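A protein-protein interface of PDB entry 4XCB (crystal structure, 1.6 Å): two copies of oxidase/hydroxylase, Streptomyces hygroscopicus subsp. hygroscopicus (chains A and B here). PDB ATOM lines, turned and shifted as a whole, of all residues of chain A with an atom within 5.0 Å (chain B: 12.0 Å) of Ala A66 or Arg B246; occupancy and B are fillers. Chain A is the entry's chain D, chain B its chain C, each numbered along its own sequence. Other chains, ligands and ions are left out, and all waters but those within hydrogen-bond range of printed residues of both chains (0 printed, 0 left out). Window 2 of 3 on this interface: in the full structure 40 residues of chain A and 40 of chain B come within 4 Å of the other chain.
Among the printed residues, pairs that only touch across the chains: Ala A66 with Arg B246, Leu A70 with Asp B244, Leu A70 with Leu B245, Leu A70 with Arg B246, Arg A87 with Thr B233, Arg A87 with Leu B245, Arg A87 with Gly B247, Arg A87 with Ala B248 and Leu A88 with Arg B246.
OG1 of Thr B242 is in hydrogen-bond range of N of Gly B247, at 3.0 Å. The backbone NH (N) of Arg B246 is in hydrogen-bond range of the side-chain hydroxyl (OG1) of Thr B242, at 3.5 Å. The backbone carbonyl oxygen (O) of Thr B233 is in hydrogen-bond range of the side-chain hydroxyl (OH) of Tyr B250, 2.6 Å away. The side-chain carboxylate (OD1) of Asp B244 lies within salt-bridge range of the guanidinium group (NE) of Arg B246 (3.98 Å). The side-chain hydroxyl (OG1) of Thr B242 is in hydrogen-bond range of the backbone NH (N) of Leu B245 (3.1 Å). The side-chain hydroxyl (OG1) of Thr B242 lies close to the backbone NH (N) of Asp B244, at 3.4 Å.
Of the printed residues of chain B, Ala A66 touches Arg B246. Arg B246 touches four residues of chain A. No residue of chain B comes within 4 Å of Pro A59. No residue of chain B comes within 4 Å of Ser A62. No residue of chain B comes within 4 Å of Pro A63. No residue of chain B comes within 4 Å of Phe A65. Arg A67 touches none of the printed residues of chain B. Leu A68 touches none of the printed residues of chain B. No residue of chain B comes within 4 Å of Ala A69. Of chain B, only Asp B244, Leu B245 and Arg B246 come within 4 Å of Leu A70. Arg A87 touches just these residues of chain B: Thr B233, Leu B245, Arg B246, Gly B247 and Ala B248. Leu A88 touches just these residues of chain B: Leu B245 (2.7 Å) and Arg B246 (3.7 Å). Printed residues of chain A within 4 Å of Asp B244: Leu A70. Of the printed residues of chain A, Leu B245 touches Leu A70, Arg A87 and Leu A88. Phe B232 touches none of the printed residues of chain A. The nearest residue of chain A that does not touch Arg B246 is Pro A59 (4.3 Å). The nearest printed residue of chain A that does not touch Leu B245 is Ala A69 (4.9 Å).
Printed residues of chain A that touch a printed residue of chain B: Ala A66, Leu A70, Arg A87 and Leu A88. Hydrophobic or aromatic side chains of chain A that line the printed part of chain B: Leu A70 and Leu A88. Among the printed residues, 11 pairs touch across the chains. Among the printed residues, no Asp or Glu carboxylate lies within 4 Å of a Lys or Arg side-chain nitrogen of the other chain.
No position is printed for both chains. Of the 11 pairs that touch across the chains among the printed residues, none has its exchanged pair printed and touching as well.
The backbone carbonyl oxygen (O) of Arg B246 is in hydrogen-bond range of the guanidinium group (NE) of Arg A87, at 3.5 Å. The backbone NH (N) of Leu A88 lies within hydrogen-bond range of the backbone carbonyl oxygen (O) of Leu B245, at 2.7 Å.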
ATOM      1  N   LEU A  58      39.271  16.220  16.043  1.00  0.00           N
ATOM      2  CA  LEU A  58      39.201  16.427  14.601  1.00  0.00           C
ATOM      3  C   LEU A  58      37.786  16.596  14.031  1.00  0.00           C
ATOM      4  O   LEU A  58      37.576  17.478  13.196  1.00  0.00           O
ATOM      5  CB  LEU A  58      39.911  15.281  13.874  1.00  0.00           C
ATOM      6  CG  LEU A  58      41.433  15.328  13.956  1.00  0.00           C
ATOM      7  CD1 LEU A  58      42.064  14.249  13.088  1.00  0.00           C
ATOM      8  CD2 LEU A  58      41.911  16.701  13.534  1.00  0.00           C
ATOM      9  N   PRO A  59      36.819  15.753  14.447  1.00  0.00           N
ATOM     10  CA  PRO A  59      35.489  15.953  13.858  1.00  0.00           C
ATOM     11  C   PRO A  59      34.890  17.329  14.158  1.00  0.00           C
ATOM     12  O   PRO A  59      34.282  17.937  13.274  1.00  0.00           O
ATOM     13  CB  PRO A  59      34.656  14.840  14.505  1.00  0.00           C
ATOM     14  CG  PRO A  59      35.653  13.763  14.797  1.00  0.00           C
ATOM     15  CD  PRO A  59      36.876  14.510  15.243  1.00  0.00           C
ATOM     16  N   SER A  62      36.967  20.152  11.848  1.00  0.00           N
ATOM     17  CA  SER A  62      36.998  20.162  10.391  1.00  0.00           C
ATOM     18  C   SER A  62      35.985  19.193   9.813  1.00  0.00           C
ATOM     19  O   SER A  62      35.895  18.048  10.253  1.00  0.00           O
ATOM     20  CB  SER A  62      38.395  19.806   9.876  1.00  0.00           C
ATOM     21  OG  SER A  62      38.390  19.631   8.468  1.00  0.00           O
ATOM     22  N   PRO A  63      35.208  19.654   8.825  1.00  0.00           N
ATOM     23  CA  PRO A  63      34.244  18.788   8.140  1.00  0.00           C
ATOM     24  C   PRO A  63      34.920  17.681   7.331  1.00  0.00           C
ATOM     25  O   PRO A  63      34.269  16.697   6.993  1.00  0.00           O
ATOM     26  CB  PRO A  63      33.491  19.759   7.223  1.00  0.00           C
ATOM     27  CG  PRO A  63      33.640  21.089   7.888  1.00  0.00           C
ATOM     28  CD  PRO A  63      35.030  21.069   8.458  1.00  0.00           C
ATOM     29  N   VAL A  64      36.203  17.834   7.024  1.00  0.00           N
ATOM     30  CA  VAL A  64      36.927  16.785   6.310  1.00  0.00           C
ATOM     31  C   VAL A  64      37.086  15.544   7.196  1.00  0.00           C
ATOM     32  O   VAL A  64      36.942  14.410   6.733  1.00  0.00           O
ATOM     33  CB  VAL A  64      38.312  17.272   5.838  1.00  0.00           C
ATOM     34  CG1 VAL A  64      39.143  16.108   5.312  1.00  0.00           C
ATOM     35  CG2 VAL A  64      38.164  18.351   4.772  1.00  0.00           C
ATOM     36  N   PHE A  65      37.366  15.778   8.476  1.00  0.00           N
ATOM     37  CA  PHE A  65      37.591  14.703   9.443  1.00  0.00           C
ATOM     38  C   PHE A  65      36.305  14.335  10.181  1.00  0.00           C
ATOM     39  O   PHE A  65      36.188  13.243  10.734  1.00  0.00           O
ATOM     40  CB  PHE A  65      38.676  15.103  10.446  1.00  0.00           C
ATOM     41  CG  PHE A  65      40.030  15.261   9.829  1.00  0.00           C
ATOM     42  CD1 PHE A  65      40.513  14.311   8.940  1.00  0.00           C
ATOM     43  CD2 PHE A  65      40.815  16.365  10.118  1.00  0.00           C
ATOM     44  CE1 PHE A  65      41.759  14.453   8.359  1.00  0.00           C
ATOM     45  CE2 PHE A  65      42.062  16.513   9.542  1.00  0.00           C
ATOM     46  CZ  PHE A  65      42.536  15.557   8.660  1.00  0.00           C
ATOM     47  N   ALA A  66      35.344  15.250  10.192  1.00  0.00           N
ATOM     48  CA  ALA A  66      34.035  14.934  10.736  1.00  0.00           C
ATOM     49  C   ALA A  66      33.361  13.872   9.870  1.00  0.00           C
ATOM     50  O   ALA A  66      32.610  13.032  10.373  1.00  0.00           O
ATOM     51  CB  ALA A  66      33.173  16.187  10.829  1.00  0.00           C
ATOM     52  N   ARG A  67      33.649  13.896   8.571  1.00  0.00           N
ATOM     53  CA  ARG A  67      33.034  12.950   7.656  1.00  0.00           C
ATOM     54  C   ARG A  67      33.907  11.718   7.476  1.00  0.00           C
ATOM     55  O   ARG A  67      33.401  10.638   7.178  1.00  0.00           O
ATOM     56  CB  ARG A  67      32.753  13.603   6.304  1.00  0.00           C
ATOM     57  CG  ARG A  67      33.970  13.860   5.450  1.00  0.00           C
ATOM     58  CD  ARG A  67      33.615  14.759   4.272  1.00  0.00           C
ATOM     59  NE  ARG A  67      33.585  16.172   4.641  1.00  0.00           N
ATOM     60  CZ  ARG A  67      33.136  17.145   3.851  1.00  0.00           C
ATOM     61  NH1 ARG A  67      32.663  16.856   2.644  1.00  0.00           N
ATOM     62  NH2 ARG A  67      33.152  18.406   4.267  1.00  0.00           N
ATOM     63  N   LEU A  68      35.216  11.870   7.657  1.00  0.00           N
ATOM     64  CA  LEU A  68      36.092  10.701   7.625  1.00  0.00           C
ATOM     65  C   LEU A  68      35.713   9.773   8.770  1.00  0.00           C
ATOM     66  O   LEU A  68      35.724   8.550   8.629  1.00  0.00           O
ATOM     67  CB  LEU A  68      37.568  11.099   7.720  1.00  0.00           C
ATOM     68  CG  LEU A  68      38.573   9.946   7.774  1.00  0.00           C
ATOM     69  CD1 LEU A  68      38.398   9.020   6.581  1.00  0.00           C
ATOM     70  CD2 LEU A  68      39.989  10.490   7.823  1.00  0.00           C
ATOM     71  N   ALA A  69      35.360  10.369   9.903  1.00  0.00           N
ATOM     72  CA  ALA A  69      34.954   9.616  11.078  1.00  0.00           C
ATOM     73  C   ALA A  69      33.762   8.702  10.782  1.00  0.00           C
ATOM     74  O   ALA A  69      33.635   7.625  11.368  1.00  0.00           O
ATOM     75  CB  ALA A  69      34.631  10.564  12.212  1.00  0.00           C
ATOM     76  N   LEU A  70      32.903   9.122   9.858  1.00  0.00           N
ATOM     77  CA  LEU A  70      31.741   8.323   9.473  1.00  0.00           C
ATOM     78  C   LEU A  70      31.960   7.623   8.133  1.00  0.00           C
ATOM     79  O   LEU A  70      31.045   7.019   7.585  1.00  0.00           O
ATOM     80  CB  LEU A  70      30.485   9.204   9.408  1.00  0.00           C
ATOM     81  CG  LEU A  70      30.159  10.014  10.667  1.00  0.00           C
ATOM     82  CD1 LEU A  70      29.050  11.034  10.417  1.00  0.00           C
ATOM     83  CD2 LEU A  70      29.782   9.092  11.806  1.00  0.00           C
ATOM     84  N   ARG A  87      28.749   3.866  17.859  1.00  0.00           N
ATOM     85  CA  ARG A  87      28.857   5.279  18.203  1.00  0.00           C
ATOM     86  C   ARG A  87      30.303   5.739  17.997  1.00  0.00           C
ATOM     87  O   ARG A  87      31.222   4.925  18.029  1.00  0.00           O
ATOM     88  CB  ARG A  87      28.419   5.524  19.649  1.00  0.00           C
ATOM     89  CG  ARG A  87      28.222   6.987  19.994  1.00  0.00           C
ATOM     90  CD  ARG A  87      28.059   7.262  21.490  1.00  0.00           C
ATOM     91  NE  ARG A  87      27.914   8.703  21.702  1.00  0.00           N
ATOM     92  CZ  ARG A  87      27.796   9.303  22.883  1.00  0.00           C
ATOM     93  NH1 ARG A  87      27.789   8.602  24.006  1.00  0.00           N
ATOM     94  NH2 ARG A  87      27.675  10.624  22.938  1.00  0.00           N
ATOM     95  N   LEU A  88      30.487   7.035  17.773  1.00  0.00           N
ATOM     96  CA  LEU A  88      31.803   7.676  17.761  1.00  0.00           C
ATOM     97  C   LEU A  88      32.248   8.081  19.155  1.00  0.00           C
ATOM     98  O   LEU A  88      31.595   8.895  19.812  1.00  0.00           O
ATOM     99  CB  LEU A  88      31.791   8.923  16.890  1.00  0.00           C
ATOM    100  CG  LEU A  88      32.593   8.935  15.601  1.00  0.00           C
ATOM    101  CD1 LEU A  88      31.853   8.119  14.585  1.00  0.00           C
ATOM    102  CD2 LEU A  88      32.758  10.371  15.133  1.00  0.00           C
ATOM    103  N   PHE B 231      32.402   4.801  32.052  1.00  0.00           N
ATOM    104  CA  PHE B 231      32.356   5.021  30.609  1.00  0.00           C
ATOM    105  C   PHE B 231      31.034   4.632  29.968  1.00  0.00           C
ATOM    106  O   PHE B 231      30.876   4.732  28.754  1.00  0.00           O
ATOM    107  CB  PHE B 231      33.493   4.258  29.911  1.00  0.00           C
ATOM    108  CG  PHE B 231      33.653   2.833  30.373  1.00  0.00           C
ATOM    109  CD1 PHE B 231      34.548   2.521  31.389  1.00  0.00           C
ATOM    110  CD2 PHE B 231      32.934   1.808  29.781  1.00  0.00           C
ATOM    111  CE1 PHE B 231      34.722   1.210  31.804  1.00  0.00           C
ATOM    112  CE2 PHE B 231      33.099   0.487  30.207  1.00  0.00           C
ATOM    113  CZ  PHE B 231      33.982   0.198  31.218  1.00  0.00           C
ATOM    114  N   PHE B 232      30.093   4.163  30.781  1.00  0.00           N
ATOM    115  CA  PHE B 232      28.733   3.918  30.313  1.00  0.00           C
ATOM    116  C   PHE B 232      27.946   5.225  30.335  1.00  0.00           C
ATOM    117  O   PHE B 232      28.116   6.016  31.252  1.00  0.00           O
ATOM    118  CB  PHE B 232      28.023   2.888  31.193  1.00  0.00           C
ATOM    119  CG  PHE B 232      28.216   1.453  30.758  1.00  0.00           C
ATOM    120  CD1 PHE B 232      29.277   1.073  29.947  1.00  0.00           C
ATOM    121  CD2 PHE B 232      27.334   0.481  31.190  1.00  0.00           C
ATOM    122  CE1 PHE B 232      29.429  -0.255  29.571  1.00  0.00           C
ATOM    123  CE2 PHE B 232      27.484  -0.832  30.815  1.00  0.00           C
ATOM    124  CZ  PHE B 232      28.541  -1.205  30.005  1.00  0.00           C
ATOM    125  N   THR B 233      27.111   5.446  29.329  1.00  0.00           N
ATOM    126  CA  THR B 233      26.170   6.591  29.371  1.00  0.00           C
ATOM    127  C   THR B 233      24.977   6.304  30.270  1.00  0.00           C
ATOM    128  O   THR B 233      24.553   5.157  30.417  1.00  0.00           O
ATOM    129  CB  THR B 233      25.643   6.960  27.981  1.00  0.00           C
ATOM    130  OG1 THR B 233      24.906   5.861  27.430  1.00  0.00           O
ATOM    131  CG2 THR B 233      26.784   7.339  27.042  1.00  0.00           C
ATOM    132  N   GLU B 234      24.420   7.363  30.857  1.00  0.00           N
ATOM    133  CA  GLU B 234      23.227   7.233  31.685  1.00  0.00           C
ATOM    134  C   GLU B 234      22.130   6.589  30.863  1.00  0.00           C
ATOM    135  O   GLU B 234      22.103   6.741  29.639  1.00  0.00           O
ATOM    136  CB  GLU B 234      22.793   8.601  32.206  1.00  0.00           C
ATOM    137  CG  GLU B 234      23.885   9.326  32.964  1.00  0.00           C
ATOM    138  CD  GLU B 234      23.461  10.710  33.432  1.00  0.00           C
ATOM    139  OE1 GLU B 234      22.588  11.322  32.781  1.00  0.00           O
ATOM    140  OE2 GLU B 234      24.002  11.177  34.456  1.00  0.00           O
ATOM    141  N   ARG B 236      19.244   5.507  28.641  1.00  0.00           N
ATOM    142  CA  ARG B 236      18.275   6.064  27.705  1.00  0.00           C
ATOM    143  C   ARG B 236      17.923   4.995  26.688  1.00  0.00           C
ATOM    144  O   ARG B 236      18.804   4.301  26.175  1.00  0.00           O
ATOM    145  CB  ARG B 236      18.824   7.299  26.987  1.00  0.00           C
ATOM    146  CG  ARG B 236      18.301   8.631  27.480  1.00  0.00           C
ATOM    147  CD  ARG B 236      19.140   9.731  26.871  1.00  0.00           C
ATOM    148  NE  ARG B 236      20.524   9.281  26.776  1.00  0.00           N
ATOM    149  CZ  ARG B 236      21.538  10.026  26.352  1.00  0.00           C
ATOM    150  NH1 ARG B 236      21.339  11.284  25.979  1.00  0.00           N
ATOM    151  NH2 ARG B 236      22.758   9.505  26.307  1.00  0.00           N
ATOM    152  N   GLU B 237      16.638   4.856  26.406  1.00  0.00           N
ATOM    153  CA  GLU B 237      16.177   3.924  25.397  1.00  0.00           C
ATOM    154  C   GLU B 237      16.554   4.428  24.011  1.00  0.00           C
ATOM    155  O   GLU B 237      16.318   5.587  23.686  1.00  0.00           O
ATOM    156  CB  GLU B 237      14.661   3.738  25.520  1.00  0.00           C
ATOM    157  CG  GLU B 237      14.065   2.774  24.524  1.00  0.00           C
ATOM    158  CD  GLU B 237      12.566   2.644  24.678  1.00  0.00           C
ATOM    159  OE1 GLU B 237      12.013   3.172  25.671  1.00  0.00           O
ATOM    160  OE2 GLU B 237      11.941   2.017  23.800  1.00  0.00           O
ATOM    161  N   LEU B 238      17.162   3.571  23.198  1.00  0.00           N
ATOM    162  CA  LEU B 238      17.523   3.941  21.833  1.00  0.00           C
ATOM    163  C   LEU B 238      16.968   2.921  20.840  1.00  0.00           C
ATOM    164  O   LEU B 238      17.081   1.714  21.056  1.00  0.00           O
ATOM    165  CB  LEU B 238      19.051   4.060  21.687  1.00  0.00           C
ATOM    166  CG  LEU B 238      19.567   4.454  20.297  1.00  0.00           C
ATOM    167  CD1 LEU B 238      19.012   5.804  19.872  1.00  0.00           C
ATOM    168  CD2 LEU B 238      21.095   4.478  20.236  1.00  0.00           C
ATOM    169  N   ASP B 239      16.368   3.408  19.756  1.00  0.00           N
ATOM    170  CA  ASP B 239      15.731   2.540  18.768  1.00  0.00           C
ATOM    171  C   ASP B 239      16.756   1.815  17.912  1.00  0.00           C
ATOM    172  O   ASP B 239      16.747   0.590  17.811  1.00  0.00           O
ATOM    173  CB  ASP B 239      14.787   3.350  17.873  1.00  0.00           C
ATOM    174  CG  ASP B 239      13.649   3.989  18.652  1.00  0.00           C
ATOM    175  OD1 ASP B 239      12.775   3.243  19.146  1.00  0.00           O
ATOM    176  OD2 ASP B 239      13.625   5.235  18.764  1.00  0.00           O
ATOM    177  N   ALA B 240      17.633   2.588  17.285  1.00  0.00           N
ATOM    178  CA  ALA B 240      18.721   2.048  16.488  1.00  0.00           C
ATOM    179  C   ALA B 240      19.882   3.021  16.532  1.00  0.00           C
ATOM    180  O   ALA B 240      19.736   4.140  17.026  1.00  0.00           O
ATOM    181  CB  ALA B 240      18.275   1.805  15.057  1.00  0.00           C
ATOM    182  N   GLU B 241      21.039   2.604  16.029  1.00  0.00           N
ATOM    183  CA  GLU B 241      22.140   3.543  15.903  1.00  0.00           C
ATOM    184  C   GLU B 241      21.735   4.640  14.926  1.00  0.00           C
ATOM    185  O   GLU B 241      21.031   4.385  13.946  1.00  0.00           O
ATOM    186  CB  GLU B 241      23.423   2.850  15.440  1.00  0.00           C
ATOM    187  CG  GLU B 241      23.383   2.328  14.021  1.00  0.00           C
ATOM    188  CD  GLU B 241      24.756   1.923  13.521  1.00  0.00           C
ATOM    189  OE1 GLU B 241      25.448   1.164  14.231  1.00  0.00           O
ATOM    190  OE2 GLU B 241      25.144   2.370  12.422  1.00  0.00           O
ATOM    191  N   THR B 242      22.156   5.865  15.215  1.00  0.00           N
ATOM    192  CA  THR B 242      21.853   6.991  14.350  1.00  0.00           C
ATOM    193  C   THR B 242      22.786   6.981  13.148  1.00  0.00           C
ATOM    194  O   THR B 242      23.851   6.366  13.189  1.00  0.00           O
ATOM    195  CB  THR B 242      21.977   8.326  15.106  1.00  0.00           C
ATOM    196  OG1 THR B 242      23.315   8.479  15.600  1.00  0.00           O
ATOM    197  CG2 THR B 242      21.009   8.358  16.281  1.00  0.00           C
ATOM    198  N   ALA B 243      22.387   7.659  12.075  1.00  0.00           N
ATOM    199  CA  ALA B 243      23.253   7.807  10.910  1.00  0.00           C
ATOM    200  C   ALA B 243      24.374   8.779  11.249  1.00  0.00           C
ATOM    201  O   ALA B 243      25.292   8.998  10.467  1.00  0.00           O
ATOM    202  CB  ALA B 243      22.463   8.289   9.704  1.00  0.00           C
ATOM    203  N   ASP B 244      24.280   9.339  12.447  1.00  0.00           N
ATOM    204  CA  ASP B 244      25.219  10.321  12.956  1.00  0.00           C
ATOM    205  C   ASP B 244      26.348   9.674  13.770  1.00  0.00           C
ATOM    206  O   ASP B 244      27.417  10.267  13.945  1.00  0.00           O
ATOM    207  CB  ASP B 244      24.464  11.327  13.820  1.00  0.00           C
ATOM    208  CG  ASP B 244      25.119  12.681  13.848  1.00  0.00           C
ATOM    209  OD1 ASP B 244      26.042  12.911  13.036  1.00  0.00           O
ATOM    210  OD2 ASP B 244      24.702  13.520  14.680  1.00  0.00           O
ATOM    211  N   LEU B 245      26.090   8.464  14.270  1.00  0.00           N
ATOM    212  CA  LEU B 245      26.955   7.782  15.243  1.00  0.00           C
ATOM    213  C   LEU B 245      27.238   8.665  16.457  1.00  0.00           C
ATOM    214  O   LEU B 245      28.197   8.439  17.188  1.00  0.00           O
ATOM    215  CB  LEU B 245      28.274   7.328  14.606  1.00  0.00           C
ATOM    216  CG  LEU B 245      28.232   6.184  13.586  1.00  0.00           C
ATOM    217  CD1 LEU B 245      29.622   5.586  13.398  1.00  0.00           C
ATOM    218  CD2 LEU B 245      27.231   5.103  13.977  1.00  0.00           C
ATOM    219  N   ARG B 246      26.403   9.674  16.681  1.00  0.00           N
ATOM    220  CA  ARG B 246      26.512  10.452  17.903  1.00  0.00           C
ATOM    221  C   ARG B 246      25.375  10.019  18.811  1.00  0.00           C
ATOM    222  O   ARG B 246      25.353  10.334  19.998  1.00  0.00           O
ATOM    223  CB  ARG B 246      26.461  11.963  17.630  1.00  0.00           C
ATOM    224  CG  ARG B 246      27.255  12.433  16.405  1.00  0.00           C
ATOM    225  CD  ARG B 246      28.739  12.090  16.457  1.00  0.00           C
ATOM    226  NE  ARG B 246      29.333  12.086  15.114  1.00  0.00           N
ATOM    227  CZ  ARG B 246      30.170  13.009  14.656  1.00  0.00           C
ATOM    228  NH1 ARG B 246      30.536  14.017  15.436  1.00  0.00           N
ATOM    229  NH2 ARG B 246      30.656  12.917  13.420  1.00  0.00           N
ATOM    230  N   GLY B 247      24.438   9.274  18.230  1.00  0.00           N
ATOM    231  CA  GLY B 247      23.309   8.734  18.966  1.00  0.00           C
ATOM    232  C   GLY B 247      23.752   7.860  20.120  1.00  0.00           C
ATOM    233  O   GLY B 247      24.455   6.856  19.928  1.00  0.00           O
ATOM    234  N   ALA B 248      23.367   8.261  21.324  1.00  0.00           N
ATOM    235  CA  ALA B 248      23.688   7.511  22.527  1.00  0.00           C
ATOM    236  C   ALA B 248      22.456   6.783  23.047  1.00  0.00           C
ATOM    237  O   ALA B 248      21.322   7.187  22.779  1.00  0.00           O
ATOM    238  CB  ALA B 248      24.249   8.427  23.595  1.00  0.00           C
ATOM    239  N   GLY B 249      22.685   5.707  23.790  1.00  0.00           N
ATOM    240  CA  GLY B 249      21.607   4.990  24.432  1.00  0.00           C
ATOM    241  C   GLY B 249      21.795   3.491  24.422  1.00  0.00           C
ATOM    242  O   GLY B 249      22.794   2.978  23.919  1.00  0.00           O
ATOM    243  N   TYR B 250      20.818   2.796  24.987  1.00  0.00           N
ATOM    244  CA  TYR B 250      20.868   1.348  25.091  1.00  0.00           C
ATOM    245  C   TYR B 250      19.833   0.729  24.156  1.00  0.00           C
ATOM    246  O   TYR B 250      18.652   1.094  24.188  1.00  0.00           O
ATOM    247  CB  TYR B 250      20.633   0.910  26.529  1.00  0.00           C
ATOM    248  CG  TYR B 250      21.692   1.365  27.509  1.00  0.00           C
ATOM    249  CD1 TYR B 250      21.811   2.705  27.880  1.00  0.00           C
ATOM    250  CD2 TYR B 250      22.568   0.452  28.079  1.00  0.00           C
ATOM    251  CE1 TYR B 250      22.776   3.116  28.784  1.00  0.00           C
ATOM    252  CE2 TYR B 250      23.529   0.850  28.982  1.00  0.00           C
ATOM    253  CZ  TYR B 250      23.645   2.181  29.323  1.00  0.00           C
ATOM    254  OH  TYR B 250      24.609   2.558  30.230  1.00  0.00           O
ATOM    255  N   VAL B 251      20.279  -0.196  23.316  1.00  0.00           N
ATOM    256  CA  VAL B 251      19.388  -0.870  22.382  1.00  0.00           C
ATOM    257  C   VAL B 251      19.176  -2.313  22.819  1.00  0.00           C
ATOM    258  O   VAL B 251      20.066  -3.150  22.687  1.00  0.00           O
ATOM    259  CB  VAL B 251      19.929  -0.847  20.949  1.00  0.00           C
ATOM    260  CG1 VAL B 251      18.883  -1.398  19.994  1.00  0.00           C
ATOM    261  CG2 VAL B 251      20.327   0.568  20.553  1.00  0.00           C
